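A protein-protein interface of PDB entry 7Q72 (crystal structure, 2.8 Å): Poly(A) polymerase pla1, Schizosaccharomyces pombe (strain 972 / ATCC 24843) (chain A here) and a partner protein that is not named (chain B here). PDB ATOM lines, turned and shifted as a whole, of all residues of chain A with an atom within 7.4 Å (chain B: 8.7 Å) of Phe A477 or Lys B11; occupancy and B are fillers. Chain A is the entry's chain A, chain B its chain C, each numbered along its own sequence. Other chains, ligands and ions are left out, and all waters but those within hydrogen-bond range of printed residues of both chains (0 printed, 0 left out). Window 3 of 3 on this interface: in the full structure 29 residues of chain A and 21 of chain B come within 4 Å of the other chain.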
ATOM      1  N   LYS A 377       4.682 -24.830  -8.596  1.00  0.00           N
ATOM      2  CA  LYS A 377       5.106 -23.733  -9.461  1.00  0.00           C
ATOM      3  C   LYS A 377       5.584 -24.227 -10.821  1.00  0.00           C
ATOM      4  O   LYS A 377       5.355 -23.562 -11.838  1.00  0.00           O
ATOM      5  CB  LYS A 377       6.209 -22.921  -8.781  1.00  0.00           C
ATOM      6  CG  LYS A 377       5.749 -22.111  -7.581  1.00  0.00           C
ATOM      7  CD  LYS A 377       6.904 -21.320  -6.984  1.00  0.00           C
ATOM      8  CE  LYS A 377       6.457 -20.501  -5.783  1.00  0.00           C
ATOM      9  NZ  LYS A 377       7.593 -19.780  -5.146  1.00  0.00           N
ATOM     10  N   TYR A 420      -3.103 -22.446 -14.282  1.00  0.00           N
ATOM     11  CA  TYR A 420      -3.496 -21.065 -14.050  1.00  0.00           C
ATOM     12  C   TYR A 420      -2.371 -20.120 -14.454  1.00  0.00           C
ATOM     13  O   TYR A 420      -1.192 -20.404 -14.225  1.00  0.00           O
ATOM     14  CB  TYR A 420      -3.857 -20.843 -12.579  1.00  0.00           C
ATOM     15  CG  TYR A 420      -5.091 -21.587 -12.120  1.00  0.00           C
ATOM     16  CD1 TYR A 420      -6.360 -21.122 -12.434  1.00  0.00           C
ATOM     17  CD2 TYR A 420      -4.988 -22.745 -11.359  1.00  0.00           C
ATOM     18  CE1 TYR A 420      -7.494 -21.791 -12.011  1.00  0.00           C
ATOM     19  CE2 TYR A 420      -6.117 -23.422 -10.932  1.00  0.00           C
ATOM     20  CZ  TYR A 420      -7.367 -22.939 -11.262  1.00  0.00           C
ATOM     21  OH  TYR A 420      -8.494 -23.607 -10.841  1.00  0.00           O
ATOM     22  N   ASN A 421      -2.745 -18.994 -15.057  1.00  0.00           N
ATOM     23  CA  ASN A 421      -1.800 -17.957 -15.469  1.00  0.00           C
ATOM     24  C   ASN A 421      -2.055 -16.722 -14.610  1.00  0.00           C
ATOM     25  O   ASN A 421      -2.753 -15.790 -15.009  1.00  0.00           O
ATOM     26  CB  ASN A 421      -1.939 -17.647 -16.967  1.00  0.00           C
ATOM     27  CG  ASN A 421      -1.441 -18.777 -17.847  1.00  0.00           C
ATOM     28  OD1 ASN A 421      -0.470 -19.457 -17.515  1.00  0.00           O
ATOM     29  ND2 ASN A 421      -2.106 -18.985 -18.978  1.00  0.00           N
ATOM     30  N   CYS A 422      -1.477 -16.723 -13.411  1.00  0.00           N
ATOM     31  CA  CYS A 422      -1.661 -15.612 -12.491  1.00  0.00           C
ATOM     32  C   CYS A 422      -0.875 -14.390 -12.954  1.00  0.00           C
ATOM     33  O   CYS A 422       0.111 -14.488 -13.690  1.00  0.00           O
ATOM     34  CB  CYS A 422      -1.231 -16.005 -11.078  1.00  0.00           C
ATOM     35  SG  CYS A 422      -2.228 -17.315 -10.339  1.00  0.00           S
ATOM     36  N   SER A 423      -1.328 -13.221 -12.505  1.00  0.00           N
ATOM     37  CA  SER A 423      -0.716 -11.946 -12.861  1.00  0.00           C
ATOM     38  C   SER A 423       0.250 -11.442 -11.795  1.00  0.00           C
ATOM     39  O   SER A 423       1.394 -11.099 -12.107  1.00  0.00           O
ATOM     40  CB  SER A 423      -1.803 -10.896 -13.116  1.00  0.00           C
ATOM     41  OG  SER A 423      -2.586 -10.686 -11.954  1.00  0.00           O
ATOM     42  N   SER A 424      -0.187 -11.390 -10.541  1.00  0.00           N
ATOM     43  CA  SER A 424       0.617 -10.867  -9.449  1.00  0.00           C
ATOM     44  C   SER A 424       1.044 -11.989  -8.512  1.00  0.00           C
ATOM     45  O   SER A 424       0.463 -13.077  -8.496  1.00  0.00           O
ATOM     46  CB  SER A 424      -0.151  -9.795  -8.667  1.00  0.00           C
ATOM     47  OG  SER A 424      -1.363 -10.313  -8.146  1.00  0.00           O
ATOM     48  N   GLU A 425       2.085 -11.705  -7.724  1.00  0.00           N
ATOM     49  CA  GLU A 425       2.572 -12.679  -6.754  1.00  0.00           C
ATOM     50  C   GLU A 425       1.554 -12.926  -5.649  1.00  0.00           C
ATOM     51  O   GLU A 425       1.462 -14.044  -5.129  1.00  0.00           O
ATOM     52  CB  GLU A 425       3.904 -12.207  -6.168  1.00  0.00           C
ATOM     53  CG  GLU A 425       4.540 -13.177  -5.182  1.00  0.00           C
ATOM     54  CD  GLU A 425       5.949 -12.771  -4.788  1.00  0.00           C
ATOM     55  OE1 GLU A 425       6.521 -11.877  -5.450  1.00  0.00           O
ATOM     56  OE2 GLU A 425       6.484 -13.345  -3.817  1.00  0.00           O
ATOM     57  N   GLU A 426       0.778 -11.903  -5.280  1.00  0.00           N
ATOM     58  CA  GLU A 426      -0.271 -12.095  -4.286  1.00  0.00           C
ATOM     59  C   GLU A 426      -1.425 -12.920  -4.840  1.00  0.00           C
ATOM     60  O   GLU A 426      -2.138 -13.578  -4.075  1.00  0.00           O
ATOM     61  CB  GLU A 426      -0.781 -10.743  -3.787  1.00  0.00           C
ATOM     62  CG  GLU A 426       0.263  -9.908  -3.063  1.00  0.00           C
ATOM     63  CD  GLU A 426      -0.278  -8.565  -2.608  1.00  0.00           C
ATOM     64  OE1 GLU A 426      -1.417  -8.222  -2.994  1.00  0.00           O
ATOM     65  OE2 GLU A 426       0.432  -7.854  -1.867  1.00  0.00           O
ATOM     66  N   GLU A 427      -1.625 -12.896  -6.159  1.00  0.00           N
ATOM     67  CA  GLU A 427      -2.712 -13.662  -6.759  1.00  0.00           C
ATOM     68  C   GLU A 427      -2.383 -15.149  -6.818  1.00  0.00           C
ATOM     69  O   GLU A 427      -3.270 -15.991  -6.642  1.00  0.00           O
ATOM     70  CB  GLU A 427      -3.022 -13.126  -8.158  1.00  0.00           C
ATOM     71  CG  GLU A 427      -4.239 -13.758  -8.816  1.00  0.00           C
ATOM     72  CD  GLU A 427      -4.573 -13.121 -10.152  1.00  0.00           C
ATOM     73  OE1 GLU A 427      -3.694 -12.449 -10.730  1.00  0.00           O
ATOM     74  OE2 GLU A 427      -5.718 -13.287 -10.620  1.00  0.00           O
ATOM     75  N   ALA A 428      -1.114 -15.489  -7.063  1.00  0.00           N
ATOM     76  CA  ALA A 428      -0.727 -16.894  -7.114  1.00  0.00           C
ATOM     77  C   ALA A 428      -0.821 -17.554  -5.745  1.00  0.00           C
ATOM     78  O   ALA A 428      -1.071 -18.762  -5.659  1.00  0.00           O
ATOM     79  CB  ALA A 428       0.687 -17.029  -7.676  1.00  0.00           C
ATOM     80  N   VAL A 431      -4.435 -18.635  -5.543  1.00  0.00           N
ATOM     81  CA  VAL A 431      -4.673 -19.835  -6.341  1.00  0.00           C
ATOM     82  C   VAL A 431      -4.102 -21.060  -5.639  1.00  0.00           C
ATOM     83  O   VAL A 431      -4.727 -22.128  -5.613  1.00  0.00           O
ATOM     84  CB  VAL A 431      -4.088 -19.657  -7.755  1.00  0.00           C
ATOM     85  CG1 VAL A 431      -3.918 -21.002  -8.440  1.00  0.00           C
ATOM     86  CG2 VAL A 431      -4.988 -18.751  -8.582  1.00  0.00           C
ATOM     87  N   PHE A 477       3.515 -15.820 -13.681  1.00  0.00           N
ATOM     88  CA  PHE A 477       3.396 -16.650 -12.487  1.00  0.00           C
ATOM     89  C   PHE A 477       2.421 -17.801 -12.716  1.00  0.00           C
ATOM     90  O   PHE A 477       1.250 -17.713 -12.344  1.00  0.00           O
ATOM     91  CB  PHE A 477       2.945 -15.808 -11.291  1.00  0.00           C
ATOM     92  CG  PHE A 477       3.898 -14.703 -10.929  1.00  0.00           C
ATOM     93  CD1 PHE A 477       5.247 -14.803 -11.232  1.00  0.00           C
ATOM     94  CD2 PHE A 477       3.446 -13.564 -10.286  1.00  0.00           C
ATOM     95  CE1 PHE A 477       6.124 -13.788 -10.900  1.00  0.00           C
ATOM     96  CE2 PHE A 477       4.316 -12.546  -9.951  1.00  0.00           C
ATOM     97  CZ  PHE A 477       5.657 -12.658 -10.258  1.00  0.00           C
ATOM     98  N   PRO A 478       2.903 -18.887 -13.324  1.00  0.00           N
ATOM     99  CA  PRO A 478       2.015 -20.014 -13.630  1.00  0.00           C
ATOM    100  C   PRO A 478       1.911 -21.005 -12.482  1.00  0.00           C
ATOM    101  O   PRO A 478       2.926 -21.426 -11.921  1.00  0.00           O
ATOM    102  CB  PRO A 478       2.673 -20.645 -14.863  1.00  0.00           C
ATOM    103  CG  PRO A 478       4.138 -20.233 -14.784  1.00  0.00           C
ATOM    104  CD  PRO A 478       4.292 -19.168 -13.720  1.00  0.00           C
ATOM    105  N   VAL A 479       0.684 -21.383 -12.128  1.00  0.00           N
ATOM    106  CA  VAL A 479       0.422 -22.339 -11.058  1.00  0.00           C
ATOM    107  C   VAL A 479      -0.289 -23.540 -11.663  1.00  0.00           C
ATOM    108  O   VAL A 479      -1.406 -23.412 -12.180  1.00  0.00           O
ATOM    109  CB  VAL A 479      -0.414 -21.718  -9.928  1.00  0.00           C
ATOM    110  CG1 VAL A 479      -0.717 -22.758  -8.861  1.00  0.00           C
ATOM    111  CG2 VAL A 479       0.312 -20.522  -9.328  1.00  0.00           C
ATOM    112  N   TYR A 480       0.353 -24.703 -11.596  1.00  0.00           N
ATOM    113  CA  TYR A 480      -0.184 -25.934 -12.160  1.00  0.00           C
ATOM    114  C   TYR A 480      -0.899 -26.718 -11.066  1.00  0.00           C
ATOM    115  O   TYR A 480      -0.360 -26.885  -9.967  1.00  0.00           O
ATOM    116  CB  TYR A 480       0.930 -26.783 -12.776  1.00  0.00           C
ATOM    117  CG  TYR A 480       1.870 -26.024 -13.690  1.00  0.00           C
ATOM    118  CD1 TYR A 480       1.420 -24.962 -14.465  1.00  0.00           C
ATOM    119  CD2 TYR A 480       3.212 -26.368 -13.774  1.00  0.00           C
ATOM    120  CE1 TYR A 480       2.282 -24.268 -15.299  1.00  0.00           C
ATOM    121  CE2 TYR A 480       4.078 -25.680 -14.605  1.00  0.00           C
ATOM    122  CZ  TYR A 480       3.609 -24.633 -15.365  1.00  0.00           C
ATOM    123  OH  TYR A 480       4.472 -23.949 -16.191  1.00  0.00           O
ATOM    124  N   SER B   6      16.653  -8.315 -18.507  1.00  0.00           N
ATOM    125  CA  SER B   6      15.252  -8.645 -18.761  1.00  0.00           C
ATOM    126  C   SER B   6      14.503  -8.627 -17.435  1.00  0.00           C
ATOM    127  O   SER B   6      14.525  -9.602 -16.681  1.00  0.00           O
ATOM    128  CB  SER B   6      15.135 -10.003 -19.445  1.00  0.00           C
ATOM    129  OG  SER B   6      15.859 -10.026 -20.663  1.00  0.00           O
ATOM    130  N   LEU B   7      13.832  -7.512 -17.151  1.00  0.00           N
ATOM    131  CA  LEU B   7      13.154  -7.365 -15.866  1.00  0.00           C
ATOM    132  C   LEU B   7      12.022  -8.366 -15.647  1.00  0.00           C
ATOM    133  O   LEU B   7      11.902  -8.871 -14.517  1.00  0.00           O
ATOM    134  CB  LEU B   7      12.642  -5.928 -15.715  1.00  0.00           C
ATOM    135  CG  LEU B   7      12.124  -5.558 -14.325  1.00  0.00           C
ATOM    136  CD1 LEU B   7      13.191  -5.808 -13.273  1.00  0.00           C
ATOM    137  CD2 LEU B   7      11.679  -4.110 -14.297  1.00  0.00           C
ATOM    138  N   PRO B   8      11.165  -8.687 -16.626  1.00  0.00           N
ATOM    139  CA  PRO B   8      10.147  -9.718 -16.362  1.00  0.00           C
ATOM    140  C   PRO B   8      10.738 -11.089 -16.086  1.00  0.00           C
ATOM    141  O   PRO B   8      10.225 -11.818 -15.227  1.00  0.00           O
ATOM    142  CB  PRO B   8       9.294  -9.707 -17.641  1.00  0.00           C
ATOM    143  CG  PRO B   8      10.173  -9.110 -18.681  1.00  0.00           C
ATOM    144  CD  PRO B   8      10.981  -8.083 -17.959  1.00  0.00           C
ATOM    145  N   LEU B   9      11.812 -11.462 -16.788  1.00  0.00           N
ATOM    146  CA  LEU B   9      12.433 -12.761 -16.548  1.00  0.00           C
ATOM    147  C   LEU B   9      13.120 -12.816 -15.189  1.00  0.00           C
ATOM    148  O   LEU B   9      13.139 -13.873 -14.549  1.00  0.00           O
ATOM    149  CB  LEU B   9      13.428 -13.087 -17.660  1.00  0.00           C
ATOM    150  CG  LEU B   9      12.823 -13.461 -19.014  1.00  0.00           C
ATOM    151  CD1 LEU B   9      13.919 -13.748 -20.029  1.00  0.00           C
ATOM    152  CD2 LEU B   9      11.893 -14.656 -18.872  1.00  0.00           C
ATOM    153  N   LEU B  10      13.692 -11.697 -14.735  1.00  0.00           N
ATOM    154  CA  LEU B  10      14.301 -11.670 -13.410  1.00  0.00           C
ATOM    155  C   LEU B  10      13.258 -11.820 -12.311  1.00  0.00           C
ATOM    156  O   LEU B  10      13.546 -12.406 -11.261  1.00  0.00           O
ATOM    157  CB  LEU B  10      15.092 -10.375 -13.219  1.00  0.00           C
ATOM    158  CG  LEU B  10      16.343 -10.213 -14.085  1.00  0.00           C
ATOM    159  CD1 LEU B  10      17.004  -8.869 -13.825  1.00  0.00           C
ATOM    160  CD2 LEU B  10      17.319 -11.354 -13.834  1.00  0.00           C
ATOM    161  N   LYS B  11      12.047 -11.298 -12.529  1.00  0.00           N
ATOM    162  CA  LYS B  11      10.983 -11.475 -11.547  1.00  0.00           C
ATOM    163  C   LYS B  11      10.482 -12.914 -11.527  1.00  0.00           C
ATOM    164  O   LYS B  11       9.995 -13.385 -10.492  1.00  0.00           O
ATOM    165  CB  LYS B  11       9.834 -10.509 -11.836  1.00  0.00           C
ATOM    166  CG  LYS B  11       9.400  -9.672 -10.640  1.00  0.00           C
ATOM    167  CD  LYS B  11       8.847 -10.539  -9.519  1.00  0.00           C
ATOM    168  CE  LYS B  11       8.384  -9.696  -8.340  1.00  0.00           C
ATOM    169  NZ  LYS B  11       7.870 -10.534  -7.219  1.00  0.00           N
ATOM    170  N   GLN B  12      10.594 -13.622 -12.651  1.00  0.00           N
ATOM    171  CA  GLN B  12      10.229 -15.035 -12.677  1.00  0.00           C
ATOM    172  C   GLN B  12      11.221 -15.870 -11.876  1.00  0.00           C
ATOM    173  O   GLN B  12      10.824 -16.724 -11.075  1.00  0.00           O
ATOM    174  CB  GLN B  12      10.150 -15.530 -14.121  1.00  0.00           C
ATOM    175  CG  GLN B  12       9.877 -17.019 -14.253  1.00  0.00           C
ATOM    176  CD  GLN B  12      10.015 -17.511 -15.680  1.00  0.00           C
ATOM    177  OE1 GLN B  12      10.198 -16.721 -16.606  1.00  0.00           O
ATOM    178  NE2 GLN B  12       9.931 -18.824 -15.865  1.00  0.00           N
ATOM    179  N   ASP B  13      12.520 -15.636 -12.081  1.00  0.00           N
ATOM    180  CA  ASP B  13      13.534 -16.367 -11.326  1.00  0.00           C
ATOM    181  C   ASP B  13      13.423 -16.075  -9.837  1.00  0.00           C
ATOM    182  O   ASP B  13      13.636 -16.965  -9.004  1.00  0.00           O
ATOM    183  CB  ASP B  13      14.929 -16.020 -11.850  1.00  0.00           C
ATOM    184  CG  ASP B  13      16.036 -16.735 -11.095  1.00  0.00           C
ATOM    185  OD1 ASP B  13      16.341 -16.336  -9.950  1.00  0.00           O
ATOM    186  OD2 ASP B  13      16.600 -17.705 -11.645  1.00  0.00           O
ATOM    187  N   ASP B  14      13.093 -14.832  -9.482  1.00  0.00           N
ATOM    188  CA  ASP B  14      12.842 -14.509  -8.082  1.00  0.00           C
ATOM    189  C   ASP B  14      11.601 -15.225  -7.563  1.00  0.00           C
ATOM    190  O   ASP B  14      11.513 -15.528  -6.368  1.00  0.00           O
ATOM    191  CB  ASP B  14      12.701 -12.996  -7.913  1.00  0.00           C
ATOM    192  CG  ASP B  14      12.516 -12.582  -6.467  1.00  0.00           C
ATOM    193  OD1 ASP B  14      13.471 -12.735  -5.675  1.00  0.00           O
ATOM    194  OD2 ASP B  14      11.415 -12.101  -6.123  1.00  0.00           O
ATOM    195  N   TRP B  15      10.640 -15.508  -8.445  1.00  0.00           N
ATOM    196  CA  TRP B  15       9.446 -16.245  -8.050  1.00  0.00           C
ATOM    197  C   TRP B  15       9.724 -17.731  -7.871  1.00  0.00           C
ATOM    198  O   TRP B  15       9.114 -18.371  -7.007  1.00  0.00           O
ATOM    199  CB  TRP B  15       8.337 -16.029  -9.084  1.00  0.00           C
ATOM    200  CG  TRP B  15       7.211 -17.015  -8.992  1.00  0.00           C
ATOM    201  CD1 TRP B  15       6.980 -18.075  -9.823  1.00  0.00           C
ATOM    202  CD2 TRP B  15       6.162 -17.035  -8.017  1.00  0.00           C
ATOM    203  NE1 TRP B  15       5.853 -18.751  -9.425  1.00  0.00           N
ATOM    204  CE2 TRP B  15       5.332 -18.132  -8.319  1.00  0.00           C
ATOM    205  CE3 TRP B  15       5.845 -16.230  -6.919  1.00  0.00           C
ATOM    206  CZ2 TRP B  15       4.206 -18.445  -7.562  1.00  0.00           C
ATOM    207  CZ3 TRP B  15       4.727 -16.543  -6.169  1.00  0.00           C
ATOM    208  CH2 TRP B  15       3.922 -17.641  -6.493  1.00  0.00           C
ATOM    209  N   LEU B  16      10.634 -18.297  -8.667  1.00  0.00           N
ATOM    210  CA  LEU B  16      10.956 -19.714  -8.529  1.00  0.00           C
ATOM    211  C   LEU B  16      11.783 -19.968  -7.274  1.00  0.00           C
ATOM    212  O   LEU B  16      11.493 -20.890  -6.502  1.00  0.00           O
ATOM    213  CB  LEU B  16      11.698 -20.207  -9.772  1.00  0.00           C
ATOM    214  CG  LEU B  16      10.961 -20.065 -11.105  1.00  0.00           C
ATOM    215  CD1 LEU B  16      11.793 -20.637 -12.242  1.00  0.00           C
ATOM    216  CD2 LEU B  16       9.599 -20.735 -11.042  1.00  0.00           C
ATOM    217  N   SER B  17      12.814 -19.157  -7.052  1.00  0.00           N
ATOM    218  CA  SER B  17      13.688 -19.299  -5.896  1.00  0.00           C
ATOM    219  C   SER B  17      13.110 -18.677  -4.632  1.00  0.00           C
ATOM    220  O   SER B  17      13.803 -18.635  -3.609  1.00  0.00           O
ATOM    221  CB  SER B  17      15.055 -18.681  -6.196  1.00  0.00           C
ATOM    222  OG  SER B  17      14.928 -17.310  -6.536  1.00  0.00           O
ATOM    223  N   SER B  18      11.868 -18.197  -4.679  1.00  0.00           N
ATOM    224  CA  SER B  18      11.256 -17.571  -3.517  1.00  0.00           C
ATOM    225  C   SER B  18      11.141 -18.565  -2.368  1.00  0.00           C
ATOM    226  O   SER B  18      10.637 -19.679  -2.539  1.00  0.00           O
ATOM    227  CB  SER B  18       9.877 -17.024  -3.883  1.00  0.00           C
ATOM    228  OG  SER B  18       9.174 -16.597  -2.729  1.00  0.00           O
ATOM    229  N   LYS B  20       9.350 -17.993   0.320  1.00  0.00           N
ATOM    230  CA  LYS B  20       8.091 -17.812   1.021  1.00  0.00           C
ATOM    231  C   LYS B  20       7.210 -19.052   0.858  1.00  0.00           C
ATOM    232  O   LYS B  20       7.297 -19.756  -0.151  1.00  0.00           O
ATOM    233  CB  LYS B  20       7.360 -16.575   0.501  1.00  0.00           C
ATOM    234  CG  LYS B  20       7.704 -15.281   1.235  1.00  0.00           C
ATOM    235  CD  LYS B  20       9.107 -14.787   0.910  1.00  0.00           C
ATOM    236  CE  LYS B  20       9.201 -14.276  -0.520  1.00  0.00           C
ATOM    237  NZ  LYS B  20      10.586 -13.849  -0.873  1.00  0.00           N
ATOM    238  N   PHE B  22       4.171 -21.503  -0.015  1.00  0.00           N
ATOM    239  CA  PHE B  22       3.219 -21.549  -1.118  1.00  0.00           C
ATOM    240  C   PHE B  22       1.841 -21.871  -0.549  1.00  0.00           C
ATOM    241  O   PHE B  22       1.585 -23.005  -0.132  1.00  0.00           O
ATOM    242  CB  PHE B  22       3.655 -22.585  -2.151  1.00  0.00           C
ATOM    243  CG  PHE B  22       3.119 -22.340  -3.532  1.00  0.00           C
ATOM    244  CD1 PHE B  22       2.379 -23.312  -4.185  1.00  0.00           C
ATOM    245  CD2 PHE B  22       3.362 -21.142  -4.181  1.00  0.00           C
ATOM    246  CE1 PHE B  22       1.892 -23.093  -5.459  1.00  0.00           C
ATOM    247  CE2 PHE B  22       2.875 -20.916  -5.454  1.00  0.00           C
ATOM    248  CZ  PHE B  22       2.138 -21.893  -6.094  1.00  0.00           C
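The side-chain carboxylate of Glu A425 is in salt-bridge range of the side-chain amino group of Lys B11 (2.6 Å).
The side-chain amino group of Lys A377 sits at hydrogen-bond distance from the backbone carbonyl oxygen of Trp B15.
The backbone NH (N) of Cys A422 sits at hydrogen-bond distance from the backbone carbonyl oxygen (O) of Phe A477 (3.1 Å).
N of Tyr A420 is in hydrogen-bond range of O of Val A479 (2.9 Å).
N of Lys B20 sits close to OG of Ser B18 (3.4 Å).
Ser B18 touches Lys A377.
CD2 of Phe B22 touches CE of Lys A377, 3.5 Å away.
Glu A425 touches Trp B15 (CG to CZ3, 3.5 Å).
Ala A428 touches Trp B15 (CB to CH2, 3.5 Å).
Phe A477 touches Lys B11 (CZ to CD, 3.9 Å).
CB of Trp B15 touches CE1 of Phe A477, 3.6 Å away.
CZ of Phe B22 touches CG2 of Val A479, at 3.96 Å.
Of chain B, only Lys B11 (3.9 Å) and Trp B15 (3.6 Å) come within 4 Å of Phe A477.
Of the printed residues of chain A, Lys B11 touches Glu A425 (2.6 Å) and Phe A477 (3.9 Å).
No residue of chain B comes within 4 Å of Cys A422.
Of the printed residues of chain B, Val A479 touches Phe B22 (3.96 Å).
Of the printed residues of chain A, Ser B18 touches Lys A377 (3.8 Å).
Of the printed residues of chain A, Phe B22 touches Lys A377 (3.5 Å) and Val A479 (3.96 Å).
Tyr A420 touches none of the printed residues of chain B.
Hydrophobic or aromatic side chains of chain B within 4 Å of the printed part of chain A: Trp B15 and Phe B22.
Of the 15 printed residues of chain A, 5 touch a printed residue of chain B.
Hydrophobic or aromatic side chains of chain A that line the printed part of chain B: Ala A428, Phe A477 and Val A479.
Among the printed residues, 9 pairs touch across the chains.
Among the printed residues, Asp or Glu carboxylates within 4 Å of a Lys or Arg side-chain nitrogen of the other chain: Glu A425 with Lys B11 (2.6 Å).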
